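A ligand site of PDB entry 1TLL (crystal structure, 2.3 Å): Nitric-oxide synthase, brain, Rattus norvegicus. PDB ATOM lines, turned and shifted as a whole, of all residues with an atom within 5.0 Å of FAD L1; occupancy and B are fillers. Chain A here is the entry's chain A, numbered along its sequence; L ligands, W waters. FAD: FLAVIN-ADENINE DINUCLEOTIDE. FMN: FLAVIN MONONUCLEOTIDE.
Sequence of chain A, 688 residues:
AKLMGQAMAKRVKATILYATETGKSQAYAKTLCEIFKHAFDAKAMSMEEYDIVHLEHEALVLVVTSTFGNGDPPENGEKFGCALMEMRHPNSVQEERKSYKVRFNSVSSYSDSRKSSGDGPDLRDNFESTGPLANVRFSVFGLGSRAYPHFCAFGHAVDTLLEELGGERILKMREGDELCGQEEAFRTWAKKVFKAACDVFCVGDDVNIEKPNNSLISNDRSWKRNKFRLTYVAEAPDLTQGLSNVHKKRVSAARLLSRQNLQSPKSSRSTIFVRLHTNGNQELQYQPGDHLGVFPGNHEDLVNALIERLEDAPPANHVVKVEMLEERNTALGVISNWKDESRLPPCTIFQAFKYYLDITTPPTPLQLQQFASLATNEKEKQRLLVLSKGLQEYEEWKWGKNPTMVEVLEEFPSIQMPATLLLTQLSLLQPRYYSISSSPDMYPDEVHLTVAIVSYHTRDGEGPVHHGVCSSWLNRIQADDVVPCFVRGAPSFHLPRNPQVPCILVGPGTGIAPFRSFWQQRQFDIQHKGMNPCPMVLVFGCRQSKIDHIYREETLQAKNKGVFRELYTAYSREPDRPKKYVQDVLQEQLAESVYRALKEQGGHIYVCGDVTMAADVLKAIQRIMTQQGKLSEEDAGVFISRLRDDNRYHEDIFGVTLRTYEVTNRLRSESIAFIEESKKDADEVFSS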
ATOM      1  N   HIS A 291     -15.420  -1.172  -1.386  1.00  0.00           N
ATOM      2  CA  HIS A 291     -15.235  -2.423  -0.645  1.00  0.00           C
ATOM      3  C   HIS A 291     -15.988  -2.390   0.653  1.00  0.00           C
ATOM      4  O   HIS A 291     -16.343  -1.316   1.156  1.00  0.00           O
ATOM      5  CB  HIS A 291     -13.758  -2.645  -0.277  1.00  0.00           C
ATOM      6  CG  HIS A 291     -12.824  -2.518  -1.438  1.00  0.00           C
ATOM      7  ND1 HIS A 291     -12.099  -1.379  -1.669  1.00  0.00           N
ATOM      8  CD2 HIS A 291     -12.543  -3.360  -2.460  1.00  0.00           C
ATOM      9  CE1 HIS A 291     -11.416  -1.517  -2.792  1.00  0.00           C
ATOM     10  NE2 HIS A 291     -11.672  -2.706  -3.294  1.00  0.00           N
ATOM     11  N   TRP A 399       7.036 -20.510   7.524  1.00  0.00           N
ATOM     12  CA  TRP A 399       6.535 -20.823   6.191  1.00  0.00           C
ATOM     13  C   TRP A 399       6.213 -22.309   5.997  1.00  0.00           C
ATOM     14  O   TRP A 399       5.421 -22.664   5.119  1.00  0.00           O
ATOM     15  CB  TRP A 399       7.550 -20.362   5.141  1.00  0.00           C
ATOM     16  CG  TRP A 399       7.628 -18.876   5.033  1.00  0.00           C
ATOM     17  CD1 TRP A 399       8.760 -18.117   5.043  1.00  0.00           C
ATOM     18  CD2 TRP A 399       6.531 -17.975   4.889  1.00  0.00           C
ATOM     19  NE1 TRP A 399       8.442 -16.791   4.902  1.00  0.00           N
ATOM     20  CE2 TRP A 399       7.077 -16.670   4.791  1.00  0.00           C
ATOM     21  CE3 TRP A 399       5.143 -18.134   4.800  1.00  0.00           C
ATOM     22  CZ2 TRP A 399       6.277 -15.531   4.646  1.00  0.00           C
ATOM     23  CZ3 TRP A 399       4.350 -17.001   4.644  1.00  0.00           C
ATOM     24  CH2 TRP A 399       4.919 -15.720   4.560  1.00  0.00           C
ATOM     25  N   ASN A 402       3.306 -22.790   9.258  1.00  0.00           N
ATOM     26  CA  ASN A 402       2.272 -21.744   9.294  1.00  0.00           C
ATOM     27  C   ASN A 402       1.500 -21.970  10.589  1.00  0.00           C
ATOM     28  O   ASN A 402       0.276 -22.078  10.585  1.00  0.00           O
ATOM     29  CB  ASN A 402       1.337 -21.900   8.080  1.00  0.00           C
ATOM     30  CG  ASN A 402       0.157 -20.932   8.129  1.00  0.00           C
ATOM     31  OD1 ASN A 402       0.331 -19.727   8.308  1.00  0.00           O
ATOM     32  ND2 ASN A 402      -1.059 -21.463   7.972  1.00  0.00           N
ATOM     33  N   ARG A 432     -11.325  -7.920   7.156  1.00  0.00           N
ATOM     34  CA  ARG A 432     -10.955  -8.282   5.797  1.00  0.00           C
ATOM     35  C   ARG A 432     -11.840  -7.514   4.811  1.00  0.00           C
ATOM     36  O   ARG A 432     -13.026  -7.294   5.071  1.00  0.00           O
ATOM     37  CB  ARG A 432     -11.127  -9.778   5.555  1.00  0.00           C
ATOM     38  CG  ARG A 432      -9.945 -10.633   5.934  1.00  0.00           C
ATOM     39  CD  ARG A 432      -9.650 -10.584   7.421  1.00  0.00           C
ATOM     40  NE  ARG A 432      -8.889 -11.754   7.826  1.00  0.00           N
ATOM     41  CZ  ARG A 432      -8.148 -11.823   8.924  1.00  0.00           C
ATOM     42  NH1 ARG A 432      -8.085 -10.783   9.738  1.00  0.00           N
ATOM     43  NH2 ARG A 432      -7.484 -12.931   9.217  1.00  0.00           N
ATOM     44  N   TYR A 433     -11.257  -7.104   3.696  1.00  0.00           N
ATOM     45  CA  TYR A 433     -11.967  -6.356   2.671  1.00  0.00           C
ATOM     46  C   TYR A 433     -12.548  -7.229   1.579  1.00  0.00           C
ATOM     47  O   TYR A 433     -11.942  -8.215   1.155  1.00  0.00           O
ATOM     48  CB  TYR A 433     -11.029  -5.342   2.048  1.00  0.00           C
ATOM     49  CG  TYR A 433     -10.648  -4.243   2.988  1.00  0.00           C
ATOM     50  CD1 TYR A 433     -11.478  -3.137   3.176  1.00  0.00           C
ATOM     51  CD2 TYR A 433      -9.463  -4.304   3.733  1.00  0.00           C
ATOM     52  CE1 TYR A 433     -11.153  -2.125   4.066  1.00  0.00           C
ATOM     53  CE2 TYR A 433      -9.123  -3.294   4.624  1.00  0.00           C
ATOM     54  CZ  TYR A 433      -9.964  -2.201   4.787  1.00  0.00           C
ATOM     55  OH  TYR A 433      -9.606  -1.170   5.643  1.00  0.00           O
ATOM     56  N   TYR A 434     -13.744  -6.870   1.128  1.00  0.00           N
ATOM     57  CA  TYR A 434     -14.446  -7.605   0.092  1.00  0.00           C
ATOM     58  C   TYR A 434     -15.100  -6.636  -0.877  1.00  0.00           C
ATOM     59  O   TYR A 434     -15.757  -5.681  -0.464  1.00  0.00           O
ATOM     60  CB  TYR A 434     -15.477  -8.513   0.730  1.00  0.00           C
ATOM     61  CG  TYR A 434     -14.837  -9.634   1.488  1.00  0.00           C
ATOM     62  CD1 TYR A 434     -14.282 -10.739   0.819  1.00  0.00           C
ATOM     63  CD2 TYR A 434     -14.698  -9.564   2.869  1.00  0.00           C
ATOM     64  CE1 TYR A 434     -13.606 -11.721   1.514  1.00  0.00           C
ATOM     65  CE2 TYR A 434     -14.028 -10.541   3.576  1.00  0.00           C
ATOM     66  CZ  TYR A 434     -13.475 -11.619   2.893  1.00  0.00           C
ATOM     67  OH  TYR A 434     -12.764 -12.541   3.639  1.00  0.00           O
ATOM     68  N   SER A 435     -14.899  -6.879  -2.178  1.00  0.00           N
ATOM     69  CA  SER A 435     -15.484  -6.021  -3.207  1.00  0.00           C
ATOM     70  C   SER A 435     -16.991  -6.206  -3.173  1.00  0.00           C
ATOM     71  O   SER A 435     -17.486  -7.329  -3.218  1.00  0.00           O
ATOM     72  CB  SER A 435     -14.974  -6.404  -4.597  1.00  0.00           C
ATOM     73  OG  SER A 435     -13.595  -6.105  -4.739  1.00  0.00           O
ATOM     74  N   THR A 450     -18.892 -11.820  -2.903  1.00  0.00           N
ATOM     75  CA  THR A 450     -18.420 -13.007  -3.621  1.00  0.00           C
ATOM     76  C   THR A 450     -17.152 -13.393  -2.830  1.00  0.00           C
ATOM     77  O   THR A 450     -16.152 -12.708  -2.878  1.00  0.00           O
ATOM     78  CB  THR A 450     -18.063 -12.618  -5.055  1.00  0.00           C
ATOM     79  OG1 THR A 450     -19.184 -11.930  -5.626  1.00  0.00           O
ATOM     80  CG2 THR A 450     -17.765 -13.826  -5.901  1.00  0.00           C
ATOM     81  N   VAL A 451     -17.216 -14.491  -2.088  1.00  0.00           N
ATOM     82  CA  VAL A 451     -16.114 -14.882  -1.234  1.00  0.00           C
ATOM     83  C   VAL A 451     -15.504 -16.266  -1.491  1.00  0.00           C
ATOM     84  O   VAL A 451     -16.155 -17.289  -1.327  1.00  0.00           O
ATOM     85  CB  VAL A 451     -16.579 -14.766   0.258  1.00  0.00           C
ATOM     86  CG1 VAL A 451     -15.476 -15.124   1.226  1.00  0.00           C
ATOM     87  CG2 VAL A 451     -17.041 -13.329   0.507  1.00  0.00           C
ATOM     88  N   ALA A 452     -14.235 -16.285  -1.928  1.00  0.00           N
ATOM     89  CA  ALA A 452     -13.543 -17.559  -2.161  1.00  0.00           C
ATOM     90  C   ALA A 452     -13.293 -18.120  -0.769  1.00  0.00           C
ATOM     91  O   ALA A 452     -12.843 -17.402   0.105  1.00  0.00           O
ATOM     92  CB  ALA A 452     -12.236 -17.317  -2.844  1.00  0.00           C
ATOM     93  N   VAL A 454     -11.161 -19.826   1.607  1.00  0.00           N
ATOM     94  CA  VAL A 454      -9.768 -20.193   1.835  1.00  0.00           C
ATOM     95  C   VAL A 454      -9.527 -21.303   2.849  1.00  0.00           C
ATOM     96  O   VAL A 454      -9.837 -21.152   4.035  1.00  0.00           O
ATOM     97  CB  VAL A 454      -8.952 -18.983   2.285  1.00  0.00           C
ATOM     98  CG1 VAL A 454      -7.586 -19.435   2.821  1.00  0.00           C
ATOM     99  CG2 VAL A 454      -8.771 -18.022   1.133  1.00  0.00           C
ATOM    100  N   TYR A 456      -6.530 -24.706   3.409  1.00  0.00           N
ATOM    101  CA  TYR A 456      -5.398 -25.424   2.836  1.00  0.00           C
ATOM    102  C   TYR A 456      -4.706 -26.288   3.879  1.00  0.00           C
ATOM    103  O   TYR A 456      -4.950 -26.136   5.089  1.00  0.00           O
ATOM    104  CB  TYR A 456      -4.389 -24.418   2.287  1.00  0.00           C
ATOM    105  CG  TYR A 456      -4.022 -23.393   3.330  1.00  0.00           C
ATOM    106  CD1 TYR A 456      -4.852 -22.290   3.580  1.00  0.00           C
ATOM    107  CD2 TYR A 456      -2.902 -23.559   4.125  1.00  0.00           C
ATOM    108  CE1 TYR A 456      -4.569 -21.388   4.593  1.00  0.00           C
ATOM    109  CE2 TYR A 456      -2.598 -22.658   5.150  1.00  0.00           C
ATOM    110  CZ  TYR A 456      -3.433 -21.576   5.372  1.00  0.00           C
ATOM    111  OH  TYR A 456      -3.145 -20.679   6.374  1.00  0.00           O
ATOM    112  N   HIS A 467      -8.077 -22.997   8.031  1.00  0.00           N
ATOM    113  CA  HIS A 467      -9.166 -22.290   7.373  1.00  0.00           C
ATOM    114  C   HIS A 467      -8.916 -20.800   7.502  1.00  0.00           C
ATOM    115  O   HIS A 467      -8.529 -20.320   8.565  1.00  0.00           O
ATOM    116  CB  HIS A 467     -10.493 -22.662   8.028  1.00  0.00           C
ATOM    117  CG  HIS A 467     -10.875 -24.090   7.837  1.00  0.00           C
ATOM    118  ND1 HIS A 467     -11.218 -24.620   6.606  1.00  0.00           N
ATOM    119  CD2 HIS A 467     -10.979 -25.117   8.723  1.00  0.00           C
ATOM    120  CE1 HIS A 467     -11.512 -25.901   6.743  1.00  0.00           C
ATOM    121  NE2 HIS A 467     -11.381 -26.228   8.019  1.00  0.00           N
ATOM    122  N   GLY A 468      -9.091 -20.078   6.401  1.00  0.00           N
ATOM    123  CA  GLY A 468      -8.925 -18.635   6.450  1.00  0.00           C
ATOM    124  C   GLY A 468      -9.919 -18.153   7.482  1.00  0.00           C
ATOM    125  O   GLY A 468     -11.023 -18.654   7.547  1.00  0.00           O
ATOM    126  N   VAL A 469      -9.535 -17.162   8.275  1.00  0.00           N
ATOM    127  CA  VAL A 469     -10.398 -16.648   9.333  1.00  0.00           C
ATOM    128  C   VAL A 469     -11.710 -16.019   8.871  1.00  0.00           C
ATOM    129  O   VAL A 469     -12.778 -16.508   9.223  1.00  0.00           O
ATOM    130  CB  VAL A 469      -9.585 -15.654  10.230  1.00  0.00           C
ATOM    131  CG1 VAL A 469     -10.493 -14.976  11.250  1.00  0.00           C
ATOM    132  CG2 VAL A 469      -8.458 -16.427  10.954  1.00  0.00           C
ATOM    133  N   CYS A 470     -11.650 -14.968   8.063  1.00  0.00           N
ATOM    134  CA  CYS A 470     -12.891 -14.314   7.591  1.00  0.00           C
ATOM    135  C   CYS A 470     -13.713 -15.173   6.628  1.00  0.00           C
ATOM    136  O   CYS A 470     -14.920 -15.315   6.802  1.00  0.00           O
ATOM    137  CB  CYS A 470     -12.577 -12.968   6.921  1.00  0.00           C
ATOM    138  SG  CYS A 470     -13.934 -11.771   6.913  1.00  0.00           S
ATOM    139  N   SER A 471     -13.081 -15.757   5.623  1.00  0.00           N
ATOM    140  CA  SER A 471     -13.836 -16.578   4.684  1.00  0.00           C
ATOM    141  C   SER A 471     -14.519 -17.756   5.365  1.00  0.00           C
ATOM    142  O   SER A 471     -15.680 -18.054   5.069  1.00  0.00           O
ATOM    143  CB  SER A 471     -12.959 -17.054   3.514  1.00  0.00           C
ATOM    144  OG  SER A 471     -11.852 -17.825   3.945  1.00  0.00           O
ATOM    145  N   SER A 472     -13.837 -18.425   6.297  1.00  0.00           N
ATOM    146  CA  SER A 472     -14.492 -19.542   6.955  1.00  0.00           C
ATOM    147  C   SER A 472     -15.607 -19.042   7.892  1.00  0.00           C
ATOM    148  O   SER A 472     -16.589 -19.727   8.128  1.00  0.00           O
ATOM    149  CB  SER A 472     -13.484 -20.395   7.733  1.00  0.00           C
ATOM    150  OG  SER A 472     -13.031 -19.720   8.877  1.00  0.00           O
ATOM    151  N   THR A 510     -12.488 -14.625  -8.006  1.00  0.00           N
ATOM    152  CA  THR A 510     -13.286 -13.645  -7.290  1.00  0.00           C
ATOM    153  C   THR A 510     -12.949 -12.213  -7.663  1.00  0.00           C
ATOM    154  O   THR A 510     -13.561 -11.259  -7.176  1.00  0.00           O
ATOM    155  CB  THR A 510     -13.207 -13.865  -5.756  1.00  0.00           C
ATOM    156  OG1 THR A 510     -11.845 -13.886  -5.324  1.00  0.00           O
ATOM    157  CG2 THR A 510     -13.869 -15.195  -5.389  1.00  0.00           C
ATOM    158  N   ALA A 513     -15.830 -10.032  -8.581  1.00  0.00           N
ATOM    159  CA  ALA A 513     -16.687  -9.416  -7.567  1.00  0.00           C
ATOM    160  C   ALA A 513     -17.219  -7.998  -7.807  1.00  0.00           C
ATOM    161  O   ALA A 513     -18.428  -7.773  -7.724  1.00  0.00           O
ATOM    162  CB  ALA A 513     -15.986  -9.454  -6.213  1.00  0.00           C
ATOM    163  N   ASP A 652      -7.607  -2.856  -8.924  1.00  0.00           N
ATOM    164  CA  ASP A 652      -8.033  -3.090  -7.552  1.00  0.00           C
ATOM    165  C   ASP A 652      -7.323  -4.366  -7.107  1.00  0.00           C
ATOM    166  O   ASP A 652      -7.759  -5.466  -7.424  1.00  0.00           O
ATOM    167  CB  ASP A 652      -9.548  -3.249  -7.448  1.00  0.00           C
ATOM    168  CG  ASP A 652     -10.032  -3.322  -5.991  1.00  0.00           C
ATOM    169  OD1 ASP A 652      -9.586  -2.483  -5.166  1.00  0.00           O
ATOM    170  OD2 ASP A 652     -10.867  -4.204  -5.659  1.00  0.00           O
ATOM    171  N   ILE A 653      -6.233  -4.195  -6.362  1.00  0.00           N
ATOM    172  CA  ILE A 653      -5.420  -5.332  -5.903  1.00  0.00           C
ATOM    173  C   ILE A 653      -5.874  -6.027  -4.634  1.00  0.00           C
ATOM    174  O   ILE A 653      -5.950  -5.417  -3.566  1.00  0.00           O
ATOM    175  CB  ILE A 653      -3.939  -4.879  -5.704  1.00  0.00           C
ATOM    176  CG1 ILE A 653      -3.449  -4.119  -6.942  1.00  0.00           C
ATOM    177  CG2 ILE A 653      -3.057  -6.085  -5.419  1.00  0.00           C
ATOM    178  CD1 ILE A 653      -3.532  -4.918  -8.218  1.00  0.00           C
ATOM    179  N   PHE A 654      -6.153  -7.316  -4.759  1.00  0.00           N
ATOM    180  CA  PHE A 654      -6.570  -8.135  -3.630  1.00  0.00           C
ATOM    181  C   PHE A 654      -5.354  -8.627  -2.851  1.00  0.00           C
ATOM    182  O   PHE A 654      -5.487  -9.161  -1.751  1.00  0.00           O
ATOM    183  CB  PHE A 654      -7.337  -9.381  -4.098  1.00  0.00           C
ATOM    184  CG  PHE A 654      -8.734  -9.113  -4.574  1.00  0.00           C
ATOM    185  CD1 PHE A 654      -9.589 -10.183  -4.808  1.00  0.00           C
ATOM    186  CD2 PHE A 654      -9.185  -7.826  -4.816  1.00  0.00           C
ATOM    187  CE1 PHE A 654     -10.865  -9.961  -5.271  1.00  0.00           C
ATOM    188  CE2 PHE A 654     -10.469  -7.609  -5.281  1.00  0.00           C
ATOM    189  CZ  PHE A 654     -11.311  -8.684  -5.505  1.00  0.00           C
ATOM    190  N   THR A 657      -3.327 -13.827  -4.022  1.00  0.00           N
ATOM    191  CA  THR A 657      -4.381 -14.812  -3.813  1.00  0.00           C
ATOM    192  C   THR A 657      -4.322 -16.023  -4.702  1.00  0.00           C
ATOM    193  O   THR A 657      -4.885 -17.054  -4.370  1.00  0.00           O
ATOM    194  CB  THR A 657      -5.793 -14.163  -3.992  1.00  0.00           C
ATOM    195  OG1 THR A 657      -5.853 -13.474  -5.244  1.00  0.00           O
ATOM    196  CG2 THR A 657      -6.077 -13.213  -2.876  1.00  0.00           C
ATOM    197  N   THR A 660      -0.759 -19.166  -4.343  1.00  0.00           N
ATOM    198  CA  THR A 660      -0.067 -18.657  -3.174  1.00  0.00           C
ATOM    199  C   THR A 660       1.193 -19.423  -2.796  1.00  0.00           C
ATOM    200  O   THR A 660       2.262 -18.835  -2.619  1.00  0.00           O
ATOM    201  CB  THR A 660      -1.002 -18.659  -1.926  1.00  0.00           C
ATOM    202  OG1 THR A 660      -2.170 -17.880  -2.213  1.00  0.00           O
ATOM    203  CG2 THR A 660      -0.290 -18.063  -0.710  1.00  0.00           C
ATOM    204  N   TYR A 661       1.065 -20.737  -2.672  1.00  0.00           N
ATOM    205  CA  TYR A 661       2.184 -21.586  -2.293  1.00  0.00           C
ATOM    206  C   TYR A 661       3.360 -21.493  -3.264  1.00  0.00           C
ATOM    207  O   TYR A 661       4.491 -21.203  -2.868  1.00  0.00           O
ATOM    208  CB  TYR A 661       1.708 -23.036  -2.213  1.00  0.00           C
ATOM    209  CG  TYR A 661       2.673 -23.950  -1.505  1.00  0.00           C
ATOM    210  CD1 TYR A 661       2.601 -24.119  -0.130  1.00  0.00           C
ATOM    211  CD2 TYR A 661       3.678 -24.610  -2.202  1.00  0.00           C
ATOM    212  CE1 TYR A 661       3.510 -24.927   0.543  1.00  0.00           C
ATOM    213  CE2 TYR A 661       4.592 -25.423  -1.541  1.00  0.00           C
ATOM    214  CZ  TYR A 661       4.501 -25.578  -0.173  1.00  0.00           C
ATOM    215  OH  TYR A 661       5.410 -26.380   0.481  1.00  0.00           O
HETATM  216  PA  FAD L   1      -6.604 -15.262   6.406  1.00  0.00           P
HETATM  217  O1A FAD L   1      -6.726 -16.178   7.438  1.00  0.00           O
HETATM  218  O2A FAD L   1      -6.151 -14.118   6.737  1.00  0.00           O
HETATM  219  O5B FAD L   1      -5.492 -16.119   5.605  1.00  0.00           O
HETATM  220  C5B FAD L   1      -4.823 -15.840   4.361  1.00  0.00           C
HETATM  221  C4B FAD L   1      -3.216 -16.086   4.583  1.00  0.00           C
HETATM  222  O4B FAD L   1      -3.157 -17.544   4.320  1.00  0.00           O
HETATM  223  C3B FAD L   1      -2.377 -15.672   3.595  1.00  0.00           C
HETATM  224  O3B FAD L   1      -1.913 -14.442   3.857  1.00  0.00           O
HETATM  225  C2B FAD L   1      -1.317 -16.691   3.474  1.00  0.00           C
HETATM  226  O2B FAD L   1      -0.178 -16.395   4.247  1.00  0.00           O
HETATM  227  C1B FAD L   1      -1.797 -17.848   3.888  1.00  0.00           C
HETATM  228  N9A FAD L   1      -2.643 -19.038   3.141  1.00  0.00           N
HETATM  229  C8A FAD L   1      -3.594 -19.103   1.964  1.00  0.00           C
HETATM  230  N7A FAD L   1      -3.472 -19.955   1.140  1.00  0.00           N
HETATM  231  C5A FAD L   1      -2.455 -20.638   1.520  1.00  0.00           C
HETATM  232  C6A FAD L   1      -1.787 -21.893   0.865  1.00  0.00           C
HETATM  233  N6A FAD L   1      -2.291 -22.462  -0.344  1.00  0.00           N
HETATM  234  N1A FAD L   1      -0.739 -22.446   1.441  1.00  0.00           N
HETATM  235  C2A FAD L   1      -0.072 -21.965   2.746  1.00  0.00           C
HETATM  236  N3A FAD L   1      -0.600 -20.769   3.474  1.00  0.00           N
HETATM  237  C4A FAD L   1      -1.836 -20.171   2.757  1.00  0.00           C
HETATM  238  N1  FAD L   1     -11.498 -11.861  -1.379  1.00  0.00           N
HETATM  239  C2  FAD L   1     -12.656 -12.363  -1.879  1.00  0.00           C
HETATM  240  O2  FAD L   1     -12.959 -13.480  -1.830  1.00  0.00           O
HETATM  241  N3  FAD L   1     -13.507 -11.496  -2.490  1.00  0.00           N
HETATM  242  C4  FAD L   1     -13.217 -10.100  -2.605  1.00  0.00           C
HETATM  243  O4  FAD L   1     -13.985  -9.463  -3.112  1.00  0.00           O
HETATM  244  C4X FAD L   1     -12.018  -9.610  -2.096  1.00  0.00           C
HETATM  245  N5  FAD L   1     -11.802  -8.217  -2.246  1.00  0.00           N
HETATM  246  C5X FAD L   1     -10.638  -7.648  -1.747  1.00  0.00           C
HETATM  247  C6  FAD L   1     -10.444  -6.330  -1.910  1.00  0.00           C
HETATM  248  C7  FAD L   1      -9.340  -5.701  -1.417  1.00  0.00           C
HETATM  249  C7M FAD L   1      -9.300  -4.247  -1.693  1.00  0.00           C
HETATM  250  C8  FAD L   1      -8.226  -6.539  -0.618  1.00  0.00           C
HETATM  251  C8M FAD L   1      -7.074  -5.931  -0.067  1.00  0.00           C
HETATM  252  C9  FAD L   1      -8.327  -7.868  -0.413  1.00  0.00           C
HETATM  253  C9A FAD L   1      -9.546  -8.520  -0.970  1.00  0.00           C
HETATM  254  N10 FAD L   1      -9.923  -9.911  -0.910  1.00  0.00           N
HETATM  255  C10 FAD L   1     -11.154 -10.485  -1.465  1.00  0.00           C
HETATM  256  C1' FAD L   1      -8.989 -10.942  -0.165  1.00  0.00           C
HETATM  257  C2' FAD L   1      -9.675 -11.017   1.345  1.00  0.00           C
HETATM  258  O2' FAD L   1      -9.835  -9.855   1.965  1.00  0.00           O
HETATM  259  C3' FAD L   1      -9.018 -12.051   2.431  1.00  0.00           C
HETATM  260  O3' FAD L   1      -7.567 -11.812   2.233  1.00  0.00           O
HETATM  261  C4' FAD L   1      -9.270 -13.409   2.162  1.00  0.00           C
HETATM  262  O4' FAD L   1     -10.818 -13.751   2.222  1.00  0.00           O
HETATM  263  C5' FAD L   1      -8.599 -14.332   3.145  1.00  0.00           C
HETATM  264  O5' FAD L   1      -8.889 -13.952   4.305  1.00  0.00           O
HETATM  265  P   FAD L   1      -9.196 -15.065   5.427  1.00  0.00           P
HETATM  266  O1P FAD L   1      -9.433 -14.040   6.286  1.00  0.00           O
HETATM  267  O2P FAD L   1     -10.062 -15.947   5.154  1.00  0.00           O
HETATM  268  O3P FAD L   1      -7.659 -15.942   5.671  1.00  0.00           O
HETATM  269  N1  FMN L   2       4.116  -4.279  -0.401  1.00  0.00           N
HETATM  270  C2  FMN L   2       4.905  -3.605  -1.243  1.00  0.00           C
HETATM  271  O2  FMN L   2       6.150  -3.468  -1.251  1.00  0.00           O
HETATM  272  N3  FMN L   2       4.194  -2.925  -2.340  1.00  0.00           N
HETATM  273  C4  FMN L   2       2.722  -2.961  -2.553  1.00  0.00           C
HETATM  274  O4  FMN L   2       2.368  -2.308  -3.568  1.00  0.00           O
HETATM  275  C4A FMN L   2       2.006  -3.669  -1.675  1.00  0.00           C
HETATM  276  N5  FMN L   2       0.698  -3.787  -1.811  1.00  0.00           N
HETATM  277  C5A FMN L   2      -0.158  -4.611  -0.900  1.00  0.00           C
HETATM  278  C6  FMN L   2      -1.584  -4.806  -1.095  1.00  0.00           C
HETATM  279  C7  FMN L   2      -2.359  -5.690  -0.167  1.00  0.00           C
HETATM  280  C7M FMN L   2      -3.747  -5.717  -0.624  1.00  0.00           C
HETATM  281  C8  FMN L   2      -1.691  -6.405   1.001  1.00  0.00           C
HETATM  282  C8M FMN L   2      -2.419  -7.312   1.946  1.00  0.00           C
HETATM  283  C9  FMN L   2      -0.328  -6.203   1.195  1.00  0.00           C
HETATM  284  C9A FMN L   2       0.551  -5.305   0.244  1.00  0.00           C
HETATM  285  N10 FMN L   2       1.999  -5.180   0.482  1.00  0.00           N
HETATM  286  C10 FMN L   2       2.759  -4.394  -0.486  1.00  0.00           C
HETATM  287  C1' FMN L   2       2.690  -5.817   1.549  1.00  0.00           C
HETATM  288  C2' FMN L   2       2.651  -4.948   2.809  1.00  0.00           C
HETATM  289  O2' FMN L   2       3.251  -3.776   2.508  1.00  0.00           O
HETATM  290  C3' FMN L   2       3.351  -5.704   3.789  1.00  0.00           C
HETATM  291  O3' FMN L   2       2.560  -6.984   4.060  1.00  0.00           O
HETATM  292  C4' FMN L   2       3.532  -5.098   5.160  1.00  0.00           C
HETATM  293  O4' FMN L   2       4.242  -6.028   5.935  1.00  0.00           O
HETATM  294  C5' FMN L   2       2.218  -4.742   5.943  1.00  0.00           C
HETATM  295  O5' FMN L   2       2.683  -3.789   6.854  1.00  0.00           O
HETATM  296  P   FMN L   2       1.687  -3.111   7.838  1.00  0.00           P
HETATM  297  O1P FMN L   2       2.436  -2.206   8.624  1.00  0.00           O
HETATM  298  O2P FMN L   2       0.677  -2.263   7.079  1.00  0.00           O
HETATM  299  O3P FMN L   2       1.229  -4.197   8.702  1.00  0.00           O
HETATM  300  O   HOH W   1      -3.209 -15.691   0.258  1.00  0.00           O
HETATM  301  O   HOH W   2      -8.318  -7.857   3.529  1.00  0.00           O
HETATM  302  O   HOH W   3      -6.022 -12.082   4.726  1.00  0.00           O
HETATM  303  O   HOH W   4       0.211 -14.412   1.545  1.00  0.00           O
HETATM  304  O   HOH W   5      -3.826 -18.233   6.966  1.00  0.00           O
HETATM  305  O   HOH W   6      -5.739 -18.876   8.954  1.00  0.00           O
HETATM  306  O   HOH W   7     -11.428 -14.973  -0.077  1.00  0.00           O
HETATM  307  O   HOH W   8      -9.815 -13.822  -3.192  1.00  0.00           O
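SG of Cys 470 sits close to OH of Tyr 434 (3.6 Å). The side-chain hydroxyl (OG) of Ser 471 lies within hydrogen-bond range of the backbone NH (N) of Val 454, 3.2 Å away. OD2 of Asp 652 is in hydrogen-bond range of OG of Ser 435, 3.4 Å away. The backbone carbonyl oxygen (O) of Val 454 sits at hydrogen-bond distance from the backbone NH (N) of Gly 468 (2.7 Å). O of Gly 468 lies within hydrogen-bond range of OG of Ser 472, 2.6 Å away. O of Val 469 is in hydrogen-bond range of OG of Ser 472 (3.2 Å). ND2 of Asn 402 sits at hydrogen-bond distance from OH of Tyr 456 (2.7 Å). OD1 of Asp 652 lies within hydrogen-bond range of NE2 of His 291, 2.8 Å away.
Water W7 lies within hydrogen-bond range of O4' of FAD L1 and O of Ala 452. Water W5 bridges OH of Tyr 456 and O4B of FAD L1. Water W2 bridges O2' of FAD L1 (3.0 Å) and N of Tyr 433 (3.0 Å). Water W8 bridges the side-chain hydroxyl of Thr 510 (2.9 Å) and a nitrogen (N1) of FAD L1 (3.2 Å). Water W6 bridges the backbone carbonyl oxygen (O) of His 467 (3.2 Å) and an oxygen (O1A) of FAD L1 (3.2 Å).
OH of Tyr 434 is in hydrogen-bond range of O4' of FAD L1, 2.7 Å away. The backbone carbonyl oxygen of Tyr 433 lies within hydrogen-bond range of an oxygen (O2') of FAD L1, 2.8 Å away. O1P of FAD L1 is in salt-bridge range of NE of Arg 432 (2.8 Å). The backbone NH (N) of Ser 471 lies within hydrogen-bond range of an oxygen (O2P) of FAD L1 (3.1 Å). O2P of FAD L1 sits at hydrogen-bond distance from OG of Ser 471, at 2.9 Å. The backbone NH (N) of Ser 435 lies within hydrogen-bond range of an oxygen (O4) of FAD L1 (2.9 Å). A nitrogen (N3) of FAD L1 is in hydrogen-bond range of the backbone carbonyl oxygen (O) of Thr 450 (2.9 Å). The backbone NH (N) of Cys 470 sits at hydrogen-bond distance from an oxygen (O1P) of FAD L1, 3.0 Å away. The backbone NH (N) of Ala 452 lies within hydrogen-bond range of an oxygen (O2) of FAD L1 (3.1 Å). O1A of FAD L1 is in hydrogen-bond range of N of Val 469, 3.1 Å away.
His 291 touches FAD L1 (NE2 to C7M, 3.3 Å). CA of Val 451 touches O2 of FAD L1, 3.5 Å away. CE2 of Tyr 456 touches N3A of FAD L1, 3.2 Å away. Gly 468 touches FAD L1. Thr 510 touches FAD L1. Ala 513 touches FAD L1. Asp 652 touches FAD L1. Ile 653 touches FAD L1 (O to C8M, 3.7 Å). Phe 654 touches FAD L1. 18 residues have an atom within 4 Å of FAD L1: His 291, Arg 432, Tyr 433, Tyr 434, Ser 435, Thr 450, Val 451, Ala 452, Tyr 456, Gly 468, Val 469, Cys 470, Ser 471, Thr 510, Ala 513, Asp 652, Ile 653 and Phe 654.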
